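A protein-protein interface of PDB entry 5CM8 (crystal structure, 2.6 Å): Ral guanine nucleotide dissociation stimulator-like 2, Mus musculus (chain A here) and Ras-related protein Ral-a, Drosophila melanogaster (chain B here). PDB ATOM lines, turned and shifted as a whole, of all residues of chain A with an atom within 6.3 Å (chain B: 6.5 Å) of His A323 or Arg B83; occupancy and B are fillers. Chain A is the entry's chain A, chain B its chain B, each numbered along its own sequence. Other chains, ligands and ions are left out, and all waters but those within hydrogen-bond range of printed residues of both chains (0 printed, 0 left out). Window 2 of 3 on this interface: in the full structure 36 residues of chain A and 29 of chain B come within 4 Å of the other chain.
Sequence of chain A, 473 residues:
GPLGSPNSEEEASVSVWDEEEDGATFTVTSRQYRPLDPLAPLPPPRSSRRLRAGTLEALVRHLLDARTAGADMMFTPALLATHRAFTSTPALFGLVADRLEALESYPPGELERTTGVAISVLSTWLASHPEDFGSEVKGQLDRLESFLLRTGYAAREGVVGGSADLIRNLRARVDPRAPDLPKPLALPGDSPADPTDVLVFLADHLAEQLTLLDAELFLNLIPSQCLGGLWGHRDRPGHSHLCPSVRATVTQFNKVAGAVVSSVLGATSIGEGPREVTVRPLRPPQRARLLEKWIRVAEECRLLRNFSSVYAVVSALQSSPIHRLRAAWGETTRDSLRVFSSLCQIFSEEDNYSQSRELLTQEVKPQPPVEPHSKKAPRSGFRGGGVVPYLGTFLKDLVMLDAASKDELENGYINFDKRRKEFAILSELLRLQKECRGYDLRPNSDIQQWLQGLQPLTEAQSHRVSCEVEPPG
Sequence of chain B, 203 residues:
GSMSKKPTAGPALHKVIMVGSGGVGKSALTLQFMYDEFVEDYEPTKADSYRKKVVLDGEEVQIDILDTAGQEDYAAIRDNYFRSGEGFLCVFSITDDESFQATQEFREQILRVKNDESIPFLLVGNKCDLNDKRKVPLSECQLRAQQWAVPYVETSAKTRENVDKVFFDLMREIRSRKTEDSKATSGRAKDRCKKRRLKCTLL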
ATOM      1  N   ALA A 316     -29.957 -21.463  23.747  1.00  0.00           N
ATOM      2  CA  ALA A 316     -29.731 -20.052  23.483  1.00  0.00           C
ATOM      3  C   ALA A 316     -29.737 -19.205  24.764  1.00  0.00           C
ATOM      4  O   ALA A 316     -28.854 -18.372  24.953  1.00  0.00           O
ATOM      5  CB  ALA A 316     -30.746 -19.537  22.487  1.00  0.00           C
ATOM      6  N   LEU A 317     -30.709 -19.435  25.648  1.00  0.00           N
ATOM      7  CA  LEU A 317     -30.782 -18.709  26.929  1.00  0.00           C
ATOM      8  C   LEU A 317     -29.668 -19.100  27.904  1.00  0.00           C
ATOM      9  O   LEU A 317     -29.388 -18.368  28.858  1.00  0.00           O
ATOM     10  CB  LEU A 317     -32.141 -18.912  27.607  1.00  0.00           C
ATOM     11  CG  LEU A 317     -33.405 -18.386  26.932  1.00  0.00           C
ATOM     12  CD1 LEU A 317     -34.620 -18.914  27.671  1.00  0.00           C
ATOM     13  CD2 LEU A 317     -33.421 -16.865  26.871  1.00  0.00           C
ATOM     14  N   GLN A 318     -29.056 -20.257  27.665  1.00  0.00           N
ATOM     15  CA  GLN A 318     -27.935 -20.739  28.468  1.00  0.00           C
ATOM     16  C   GLN A 318     -26.582 -20.451  27.819  1.00  0.00           C
ATOM     17  O   GLN A 318     -25.543 -20.682  28.425  1.00  0.00           O
ATOM     18  CB  GLN A 318     -28.070 -22.247  28.732  1.00  0.00           C
ATOM     19  CG  GLN A 318     -28.859 -22.600  29.979  1.00  0.00           C
ATOM     20  CD  GLN A 318     -28.865 -24.094  30.276  1.00  0.00           C
ATOM     21  OE1 GLN A 318     -29.064 -24.921  29.385  1.00  0.00           O
ATOM     22  NE2 GLN A 318     -28.657 -24.443  31.538  1.00  0.00           N
ATOM     23  N   SER A 319     -26.598 -19.956  26.584  1.00  0.00           N
ATOM     24  CA  SER A 319     -25.362 -19.652  25.864  1.00  0.00           C
ATOM     25  C   SER A 319     -24.649 -18.459  26.496  1.00  0.00           C
ATOM     26  O   SER A 319     -25.277 -17.647  27.183  1.00  0.00           O
ATOM     27  CB  SER A 319     -25.638 -19.402  24.381  1.00  0.00           C
ATOM     28  OG  SER A 319     -26.298 -18.167  24.184  1.00  0.00           O
ATOM     29  N   SER A 320     -23.344 -18.358  26.252  1.00  0.00           N
ATOM     30  CA  SER A 320     -22.483 -17.421  26.983  1.00  0.00           C
ATOM     31  C   SER A 320     -22.876 -15.941  26.885  1.00  0.00           C
ATOM     32  O   SER A 320     -22.894 -15.267  27.908  1.00  0.00           O
ATOM     33  CB  SER A 320     -20.996 -17.646  26.669  1.00  0.00           C
ATOM     34  OG  SER A 320     -20.707 -17.407  25.305  1.00  0.00           O
ATOM     35  N   PRO A 321     -23.218 -15.437  25.677  1.00  0.00           N
ATOM     36  CA  PRO A 321     -23.596 -14.015  25.604  1.00  0.00           C
ATOM     37  C   PRO A 321     -24.938 -13.664  26.268  1.00  0.00           C
ATOM     38  O   PRO A 321     -25.255 -12.479  26.417  1.00  0.00           O
ATOM     39  CB  PRO A 321     -23.674 -13.748  24.097  1.00  0.00           C
ATOM     40  CG  PRO A 321     -23.950 -15.068  23.490  1.00  0.00           C
ATOM     41  CD  PRO A 321     -23.234 -16.071  24.341  1.00  0.00           C
ATOM     42  N   ILE A 322     -25.719 -14.672  26.650  1.00  0.00           N
ATOM     43  CA  ILE A 322     -27.004 -14.425  27.305  1.00  0.00           C
ATOM     44  C   ILE A 322     -26.917 -14.750  28.794  1.00  0.00           C
ATOM     45  O   ILE A 322     -27.526 -14.067  29.620  1.00  0.00           O
ATOM     46  CB  ILE A 322     -28.173 -15.200  26.616  1.00  0.00           C
ATOM     47  CG1 ILE A 322     -28.258 -14.860  25.120  1.00  0.00           C
ATOM     48  CG2 ILE A 322     -29.510 -14.937  27.316  1.00  0.00           C
ATOM     49  CD1 ILE A 322     -28.415 -13.371  24.793  1.00  0.00           C
ATOM     50  N   HIS A 323     -26.143 -15.783  29.119  1.00  0.00           N
ATOM     51  CA  HIS A 323     -25.872 -16.183  30.498  1.00  0.00           C
ATOM     52  C   HIS A 323     -25.105 -15.102  31.276  1.00  0.00           C
ATOM     53  O   HIS A 323     -25.220 -15.006  32.503  1.00  0.00           O
ATOM     54  CB  HIS A 323     -25.089 -17.492  30.496  1.00  0.00           C
ATOM     55  CG  HIS A 323     -25.061 -18.188  31.818  1.00  0.00           C
ATOM     56  ND1 HIS A 323     -24.060 -17.987  32.746  1.00  0.00           N
ATOM     57  CD2 HIS A 323     -25.901 -19.100  32.362  1.00  0.00           C
ATOM     58  CE1 HIS A 323     -24.291 -18.740  33.808  1.00  0.00           C
ATOM     59  NE2 HIS A 323     -25.402 -19.425  33.600  1.00  0.00           N
ATOM     60  N   ARG A 324     -24.326 -14.296  30.556  1.00  0.00           N
ATOM     61  CA  ARG A 324     -23.572 -13.189  31.147  1.00  0.00           C
ATOM     62  C   ARG A 324     -24.456 -12.083  31.716  1.00  0.00           C
ATOM     63  O   ARG A 324     -24.078 -11.436  32.689  1.00  0.00           O
ATOM     64  CB  ARG A 324     -22.650 -12.556  30.110  1.00  0.00           C
ATOM     65  CG  ARG A 324     -21.330 -13.257  29.883  1.00  0.00           C
ATOM     66  CD  ARG A 324     -20.233 -12.256  29.533  1.00  0.00           C
ATOM     67  NE  ARG A 324     -20.759 -11.027  28.939  1.00  0.00           N
ATOM     68  CZ  ARG A 324     -20.858  -9.861  29.576  1.00  0.00           C
ATOM     69  NH1 ARG A 324     -20.458  -9.741  30.837  1.00  0.00           N
ATOM     70  NH2 ARG A 324     -21.359  -8.810  28.945  1.00  0.00           N
ATOM     71  N   LEU A 325     -25.615 -11.859  31.097  1.00  0.00           N
ATOM     72  CA  LEU A 325     -26.482 -10.723  31.432  1.00  0.00           C
ATOM     73  C   LEU A 325     -27.141 -10.872  32.806  1.00  0.00           C
ATOM     74  O   LEU A 325     -28.325 -11.202  32.913  1.00  0.00           O
ATOM     75  CB  LEU A 325     -27.545 -10.510  30.346  1.00  0.00           C
ATOM     76  CG  LEU A 325     -27.143 -10.502  28.867  1.00  0.00           C
ATOM     77  CD1 LEU A 325     -28.376 -10.698  27.990  1.00  0.00           C
ATOM     78  CD2 LEU A 325     -26.397  -9.228  28.474  1.00  0.00           C
ATOM     79  N   ARG A 326     -26.360 -10.613  33.854  1.00  0.00           N
ATOM     80  CA  ARG A 326     -26.798 -10.824  35.231  1.00  0.00           C
ATOM     81  C   ARG A 326     -27.879  -9.845  35.684  1.00  0.00           C
ATOM     82  O   ARG A 326     -28.758 -10.211  36.470  1.00  0.00           O
ATOM     83  CB  ARG A 326     -25.601 -10.789  36.188  1.00  0.00           C
ATOM     84  CG  ARG A 326     -24.703 -12.040  36.142  1.00  0.00           C
ATOM     85  CD  ARG A 326     -25.422 -13.309  36.654  1.00  0.00           C
ATOM     86  NE  ARG A 326     -25.966 -14.138  35.573  1.00  0.00           N
ATOM     87  CZ  ARG A 326     -26.805 -15.164  35.741  1.00  0.00           C
ATOM     88  NH1 ARG A 326     -27.230 -15.503  36.954  1.00  0.00           N
ATOM     89  NH2 ARG A 326     -27.232 -15.853  34.685  1.00  0.00           N
ATOM     90  N   TRP A 329     -31.250 -11.028  34.078  1.00  0.00           N
ATOM     91  CA  TRP A 329     -31.758 -12.178  34.815  1.00  0.00           C
ATOM     92  C   TRP A 329     -32.280 -11.761  36.184  1.00  0.00           C
ATOM     93  O   TRP A 329     -33.249 -12.340  36.686  1.00  0.00           O
ATOM     94  CB  TRP A 329     -30.691 -13.273  34.942  1.00  0.00           C
ATOM     95  CG  TRP A 329     -30.443 -14.025  33.659  1.00  0.00           C
ATOM     96  CD1 TRP A 329     -29.336 -13.947  32.861  1.00  0.00           C
ATOM     97  CD2 TRP A 329     -31.328 -14.955  33.020  1.00  0.00           C
ATOM     98  NE1 TRP A 329     -29.475 -14.771  31.771  1.00  0.00           N
ATOM     99  CE2 TRP A 329     -30.688 -15.402  31.842  1.00  0.00           C
ATOM    100  CE3 TRP A 329     -32.603 -15.452  33.325  1.00  0.00           C
ATOM    101  CZ2 TRP A 329     -31.277 -16.325  30.972  1.00  0.00           C
ATOM    102  CZ3 TRP A 329     -33.187 -16.374  32.461  1.00  0.00           C
ATOM    103  CH2 TRP A 329     -32.521 -16.800  31.299  1.00  0.00           C
ATOM    104  N   GLU A 349     -27.388 -32.978  30.114  1.00  0.00           N
ATOM    105  CA  GLU A 349     -26.605 -34.082  29.570  1.00  0.00           C
ATOM    106  C   GLU A 349     -26.490 -35.226  30.570  1.00  0.00           C
ATOM    107  O   GLU A 349     -26.087 -36.334  30.211  1.00  0.00           O
ATOM    108  CB  GLU A 349     -25.202 -33.603  29.185  1.00  0.00           C
ATOM    109  CG  GLU A 349     -25.097 -32.116  28.863  1.00  0.00           C
ATOM    110  CD  GLU A 349     -24.965 -31.247  30.107  1.00  0.00           C
ATOM    111  OE1 GLU A 349     -24.618 -31.781  31.185  1.00  0.00           O
ATOM    112  OE2 GLU A 349     -25.209 -30.026  30.002  1.00  0.00           O
ATOM    113  N   ARG B  78     -23.097 -26.249  22.947  1.00  0.00           N
ATOM    114  CA  ARG B  78     -21.783 -26.495  23.547  1.00  0.00           C
ATOM    115  C   ARG B  78     -21.462 -25.562  24.713  1.00  0.00           C
ATOM    116  O   ARG B  78     -20.762 -25.957  25.645  1.00  0.00           O
ATOM    117  CB  ARG B  78     -20.669 -26.459  22.499  1.00  0.00           C
ATOM    118  CG  ARG B  78     -20.344 -25.082  21.919  1.00  0.00           C
ATOM    119  CD  ARG B  78     -19.583 -25.243  20.616  1.00  0.00           C
ATOM    120  NE  ARG B  78     -20.416 -25.920  19.626  1.00  0.00           N
ATOM    121  CZ  ARG B  78     -19.985 -26.825  18.753  1.00  0.00           C
ATOM    122  NH1 ARG B  78     -18.706 -27.188  18.729  1.00  0.00           N
ATOM    123  NH2 ARG B  78     -20.846 -27.373  17.904  1.00  0.00           N
ATOM    124  N   ASP B  79     -21.984 -24.337  24.656  1.00  0.00           N
ATOM    125  CA  ASP B  79     -21.786 -23.354  25.719  1.00  0.00           C
ATOM    126  C   ASP B  79     -22.130 -23.917  27.098  1.00  0.00           C
ATOM    127  O   ASP B  79     -21.444 -23.637  28.080  1.00  0.00           O
ATOM    128  CB  ASP B  79     -22.610 -22.094  25.448  1.00  0.00           C
ATOM    129  CG  ASP B  79     -22.052 -21.256  24.310  1.00  0.00           C
ATOM    130  OD1 ASP B  79     -21.529 -21.824  23.326  1.00  0.00           O
ATOM    131  OD2 ASP B  79     -22.149 -20.016  24.398  1.00  0.00           O
ATOM    132  N   ASN B  80     -23.189 -24.719  27.158  1.00  0.00           N
ATOM    133  CA  ASN B  80     -23.605 -25.351  28.402  1.00  0.00           C
ATOM    134  C   ASN B  80     -22.846 -26.651  28.691  1.00  0.00           C
ATOM    135  O   ASN B  80     -22.745 -27.070  29.842  1.00  0.00           O
ATOM    136  CB  ASN B  80     -25.114 -25.593  28.393  1.00  0.00           C
ATOM    137  CG  ASN B  80     -25.652 -25.978  29.756  1.00  0.00           C
ATOM    138  OD1 ASN B  80     -25.681 -25.165  30.682  1.00  0.00           O
ATOM    139  ND2 ASN B  80     -26.087 -27.227  29.885  1.00  0.00           N
ATOM    140  N   TYR B  81     -22.320 -27.289  27.648  1.00  0.00           N
ATOM    141  CA  TYR B  81     -21.468 -28.464  27.824  1.00  0.00           C
ATOM    142  C   TYR B  81     -20.189 -28.033  28.538  1.00  0.00           C
ATOM    143  O   TYR B  81     -19.786 -28.646  29.530  1.00  0.00           O
ATOM    144  CB  TYR B  81     -21.132 -29.113  26.474  1.00  0.00           C
ATOM    145  CG  TYR B  81     -22.280 -29.825  25.769  1.00  0.00           C
ATOM    146  CD1 TYR B  81     -23.613 -29.524  26.054  1.00  0.00           C
ATOM    147  CD2 TYR B  81     -22.023 -30.784  24.789  1.00  0.00           C
ATOM    148  CE1 TYR B  81     -24.656 -30.165  25.397  1.00  0.00           C
ATOM    149  CE2 TYR B  81     -23.060 -31.435  24.126  1.00  0.00           C
ATOM    150  CZ  TYR B  81     -24.372 -31.117  24.434  1.00  0.00           C
ATOM    151  OH  TYR B  81     -25.407 -31.758  23.782  1.00  0.00           O
ATOM    152  N   PHE B  82     -19.575 -26.960  28.037  1.00  0.00           N
ATOM    153  CA  PHE B  82     -18.370 -26.392  28.641  1.00  0.00           C
ATOM    154  C   PHE B  82     -18.648 -25.811  30.023  1.00  0.00           C
ATOM    155  O   PHE B  82     -17.822 -25.940  30.923  1.00  0.00           O
ATOM    156  CB  PHE B  82     -17.746 -25.314  27.745  1.00  0.00           C
ATOM    157  CG  PHE B  82     -17.533 -25.741  26.318  1.00  0.00           C
ATOM    158  CD1 PHE B  82     -17.659 -24.818  25.289  1.00  0.00           C
ATOM    159  CD2 PHE B  82     -17.213 -27.059  25.999  1.00  0.00           C
ATOM    160  CE1 PHE B  82     -17.466 -25.193  23.964  1.00  0.00           C
ATOM    161  CE2 PHE B  82     -17.027 -27.446  24.677  1.00  0.00           C
ATOM    162  CZ  PHE B  82     -17.153 -26.509  23.657  1.00  0.00           C
ATOM    163  N   ARG B  83     -19.808 -25.171  30.175  1.00  0.00           N
ATOM    164  CA  ARG B  83     -20.255 -24.619  31.455  1.00  0.00           C
ATOM    165  C   ARG B  83     -21.405 -25.456  32.038  1.00  0.00           C
ATOM    166  O   ARG B  83     -22.572 -25.258  31.677  1.00  0.00           O
ATOM    167  CB  ARG B  83     -20.721 -23.177  31.279  1.00  0.00           C
ATOM    168  CG  ARG B  83     -21.014 -22.431  32.573  1.00  0.00           C
ATOM    169  CD  ARG B  83     -22.390 -21.763  32.554  1.00  0.00           C
ATOM    170  NE  ARG B  83     -22.865 -21.394  31.217  1.00  0.00           N
ATOM    171  CZ  ARG B  83     -22.563 -20.260  30.587  1.00  0.00           C
ATOM    172  NH1 ARG B  83     -21.762 -19.363  31.151  1.00  0.00           N
ATOM    173  NH2 ARG B  83     -23.057 -20.028  29.378  1.00  0.00           N
ATOM    174  N   SER B  84     -21.085 -26.369  32.953  1.00  0.00           N
ATOM    175  CA  SER B  84     -19.725 -26.538  33.435  1.00  0.00           C
ATOM    176  C   SER B  84     -19.216 -27.970  33.286  1.00  0.00           C
ATOM    177  O   SER B  84     -19.826 -28.926  33.779  1.00  0.00           O
ATOM    178  CB  SER B  84     -19.582 -26.035  34.881  1.00  0.00           C
ATOM    179  OG  SER B  84     -20.755 -26.272  35.640  1.00  0.00           O
ATOM    180  N   GLY B  85     -18.104 -28.092  32.566  1.00  0.00           N
ATOM    181  CA  GLY B  85     -17.344 -29.327  32.471  1.00  0.00           C
ATOM    182  C   GLY B  85     -15.982 -29.096  33.093  1.00  0.00           C
ATOM    183  O   GLY B  85     -15.342 -28.072  32.845  1.00  0.00           O
ATOM    184  N   PHE B  88     -11.119 -30.830  29.846  1.00  0.00           N
ATOM    185  CA  PHE B  88     -11.240 -30.555  28.412  1.00  0.00           C
ATOM    186  C   PHE B  88     -10.163 -31.235  27.569  1.00  0.00           C
ATOM    187  O   PHE B  88      -8.972 -31.134  27.866  1.00  0.00           O
ATOM    188  CB  PHE B  88     -11.232 -29.044  28.149  1.00  0.00           C
ATOM    189  CG  PHE B  88     -12.408 -28.319  28.734  1.00  0.00           C
ATOM    190  CD1 PHE B  88     -12.306 -27.686  29.969  1.00  0.00           C
ATOM    191  CD2 PHE B  88     -13.618 -28.267  28.051  1.00  0.00           C
ATOM    192  CE1 PHE B  88     -13.391 -27.012  30.518  1.00  0.00           C
ATOM    193  CE2 PHE B  88     -14.711 -27.594  28.590  1.00  0.00           C
ATOM    194  CZ  PHE B  88     -14.598 -26.965  29.827  1.00  0.00           C
ATOM    195  N   ARG B 112     -14.557 -18.302  26.391  1.00  0.00           N
ATOM    196  CA  ARG B 112     -15.676 -17.367  26.313  1.00  0.00           C
ATOM    197  C   ARG B 112     -16.763 -17.761  27.321  1.00  0.00           C
ATOM    198  O   ARG B 112     -17.741 -17.033  27.514  1.00  0.00           O
ATOM    199  CB  ARG B 112     -16.231 -17.340  24.885  1.00  0.00           C
ATOM    200  CG  ARG B 112     -16.963 -16.060  24.506  1.00  0.00           C
ATOM    201  CD  ARG B 112     -16.978 -15.850  22.994  1.00  0.00           C
ATOM    202  NE  ARG B 112     -15.686 -15.377  22.494  1.00  0.00           N
ATOM    203  CZ  ARG B 112     -15.437 -15.035  21.231  1.00  0.00           C
ATOM    204  NH1 ARG B 112     -16.389 -15.107  20.309  1.00  0.00           N
ATOM    205  NH2 ARG B 112     -14.227 -14.618  20.887  1.00  0.00           N
ATOM    206  N   VAL B 113     -16.567 -18.912  27.965  1.00  0.00           N
ATOM    207  CA  VAL B 113     -17.509 -19.452  28.945  1.00  0.00           C
ATOM    208  C   VAL B 113     -16.863 -19.593  30.336  1.00  0.00           C
ATOM    209  O   VAL B 113     -17.559 -19.631  31.353  1.00  0.00           O
ATOM    210  CB  VAL B 113     -18.095 -20.816  28.486  1.00  0.00           C
ATOM    211  CG1 VAL B 113     -19.381 -21.106  29.214  1.00  0.00           C
ATOM    212  CG2 VAL B 113     -18.365 -20.823  26.989  1.00  0.00           C
ATOM    213  N   LYS B 114     -15.534 -19.670  30.366  1.00  0.00           N
ATOM    214  CA  LYS B 114     -14.776 -19.749  31.616  1.00  0.00           C
ATOM    215  C   LYS B 114     -13.788 -18.585  31.721  1.00  0.00           C
ATOM    216  O   LYS B 114     -13.158 -18.212  30.732  1.00  0.00           O
ATOM    217  CB  LYS B 114     -14.004 -21.071  31.696  1.00  0.00           C
ATOM    218  CG  LYS B 114     -14.837 -22.334  31.522  1.00  0.00           C
ATOM    219  CD  LYS B 114     -15.461 -22.785  32.829  1.00  0.00           C
ATOM    220  CE  LYS B 114     -15.823 -24.259  32.769  1.00  0.00           C
ATOM    221  NZ  LYS B 114     -16.436 -24.747  34.031  1.00  0.00           N
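Hydrophobic or aromatic side chains of chain A within 4 Å of the printed part of chain B: His A323.
Among the printed residues, 9 pairs touch across the chains.
Among the printed residues, no Asp or Glu carboxylate lies within 4 Å of a Lys or Arg side-chain nitrogen of the other chain.
Among the printed residues, merely in contact across the chains: Ser A320 with Arg B112 (3.4 Å), Ser A319 with Asp B79 (3.5 Å), Ser A320 with Arg B83 (3.6 Å) and Ser A319 with Arg B83 (3.6 Å).
The side-chain hydroxyl (OG) of Ser A319 lies within hydrogen-bond range of the backbone carbonyl oxygen (O) of Ala A316 (2.7 Å).
O of His A323 is in hydrogen-bond range of NH2 of Arg A326 (3.1 Å).
The backbone carbonyl oxygen (O) of Arg B83 sits close to the side-chain amide oxygen (OD1) of Asn B80.
Printed residues of chain B within 4 Å of His A323: Arg B83 (3.1 Å).
Printed residues of chain A within 4 Å of Arg B83: Gln A318, Ser A319, Ser A320 and His A323.
Of the printed residues of chain A, Arg B112 touches Ser A320 (3.4 Å).
Printed residues of chain A within 4 Å of Asn B80: Gln A318 (3.2 Å) and Glu A349 (2.9 Å).
The nearest printed residue of chain A that does not touch Arg B83 is Glu A349 (5.7 Å).
NE2 of Gln A318 lies within hydrogen-bond range of OD1 of Asn B80, 3.2 Å away.
The backbone carbonyl oxygen (O) of Gln A318 is in hydrogen-bond range of the guanidinium group (NH2) of Arg B83, at 2.7 Å.
The backbone NH (N) of Ser A320 sits at hydrogen-bond distance from the side-chain carboxylate (OD2) of Asp B79.
NH1 of Arg B83 sits at hydrogen-bond distance from ND1 of His A323 (3.1 Å).
The side-chain amide nitrogen (ND2) of Asn B80 lies within hydrogen-bond range of the side-chain carboxylate (OE2) of Glu A349 (2.9 Å).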
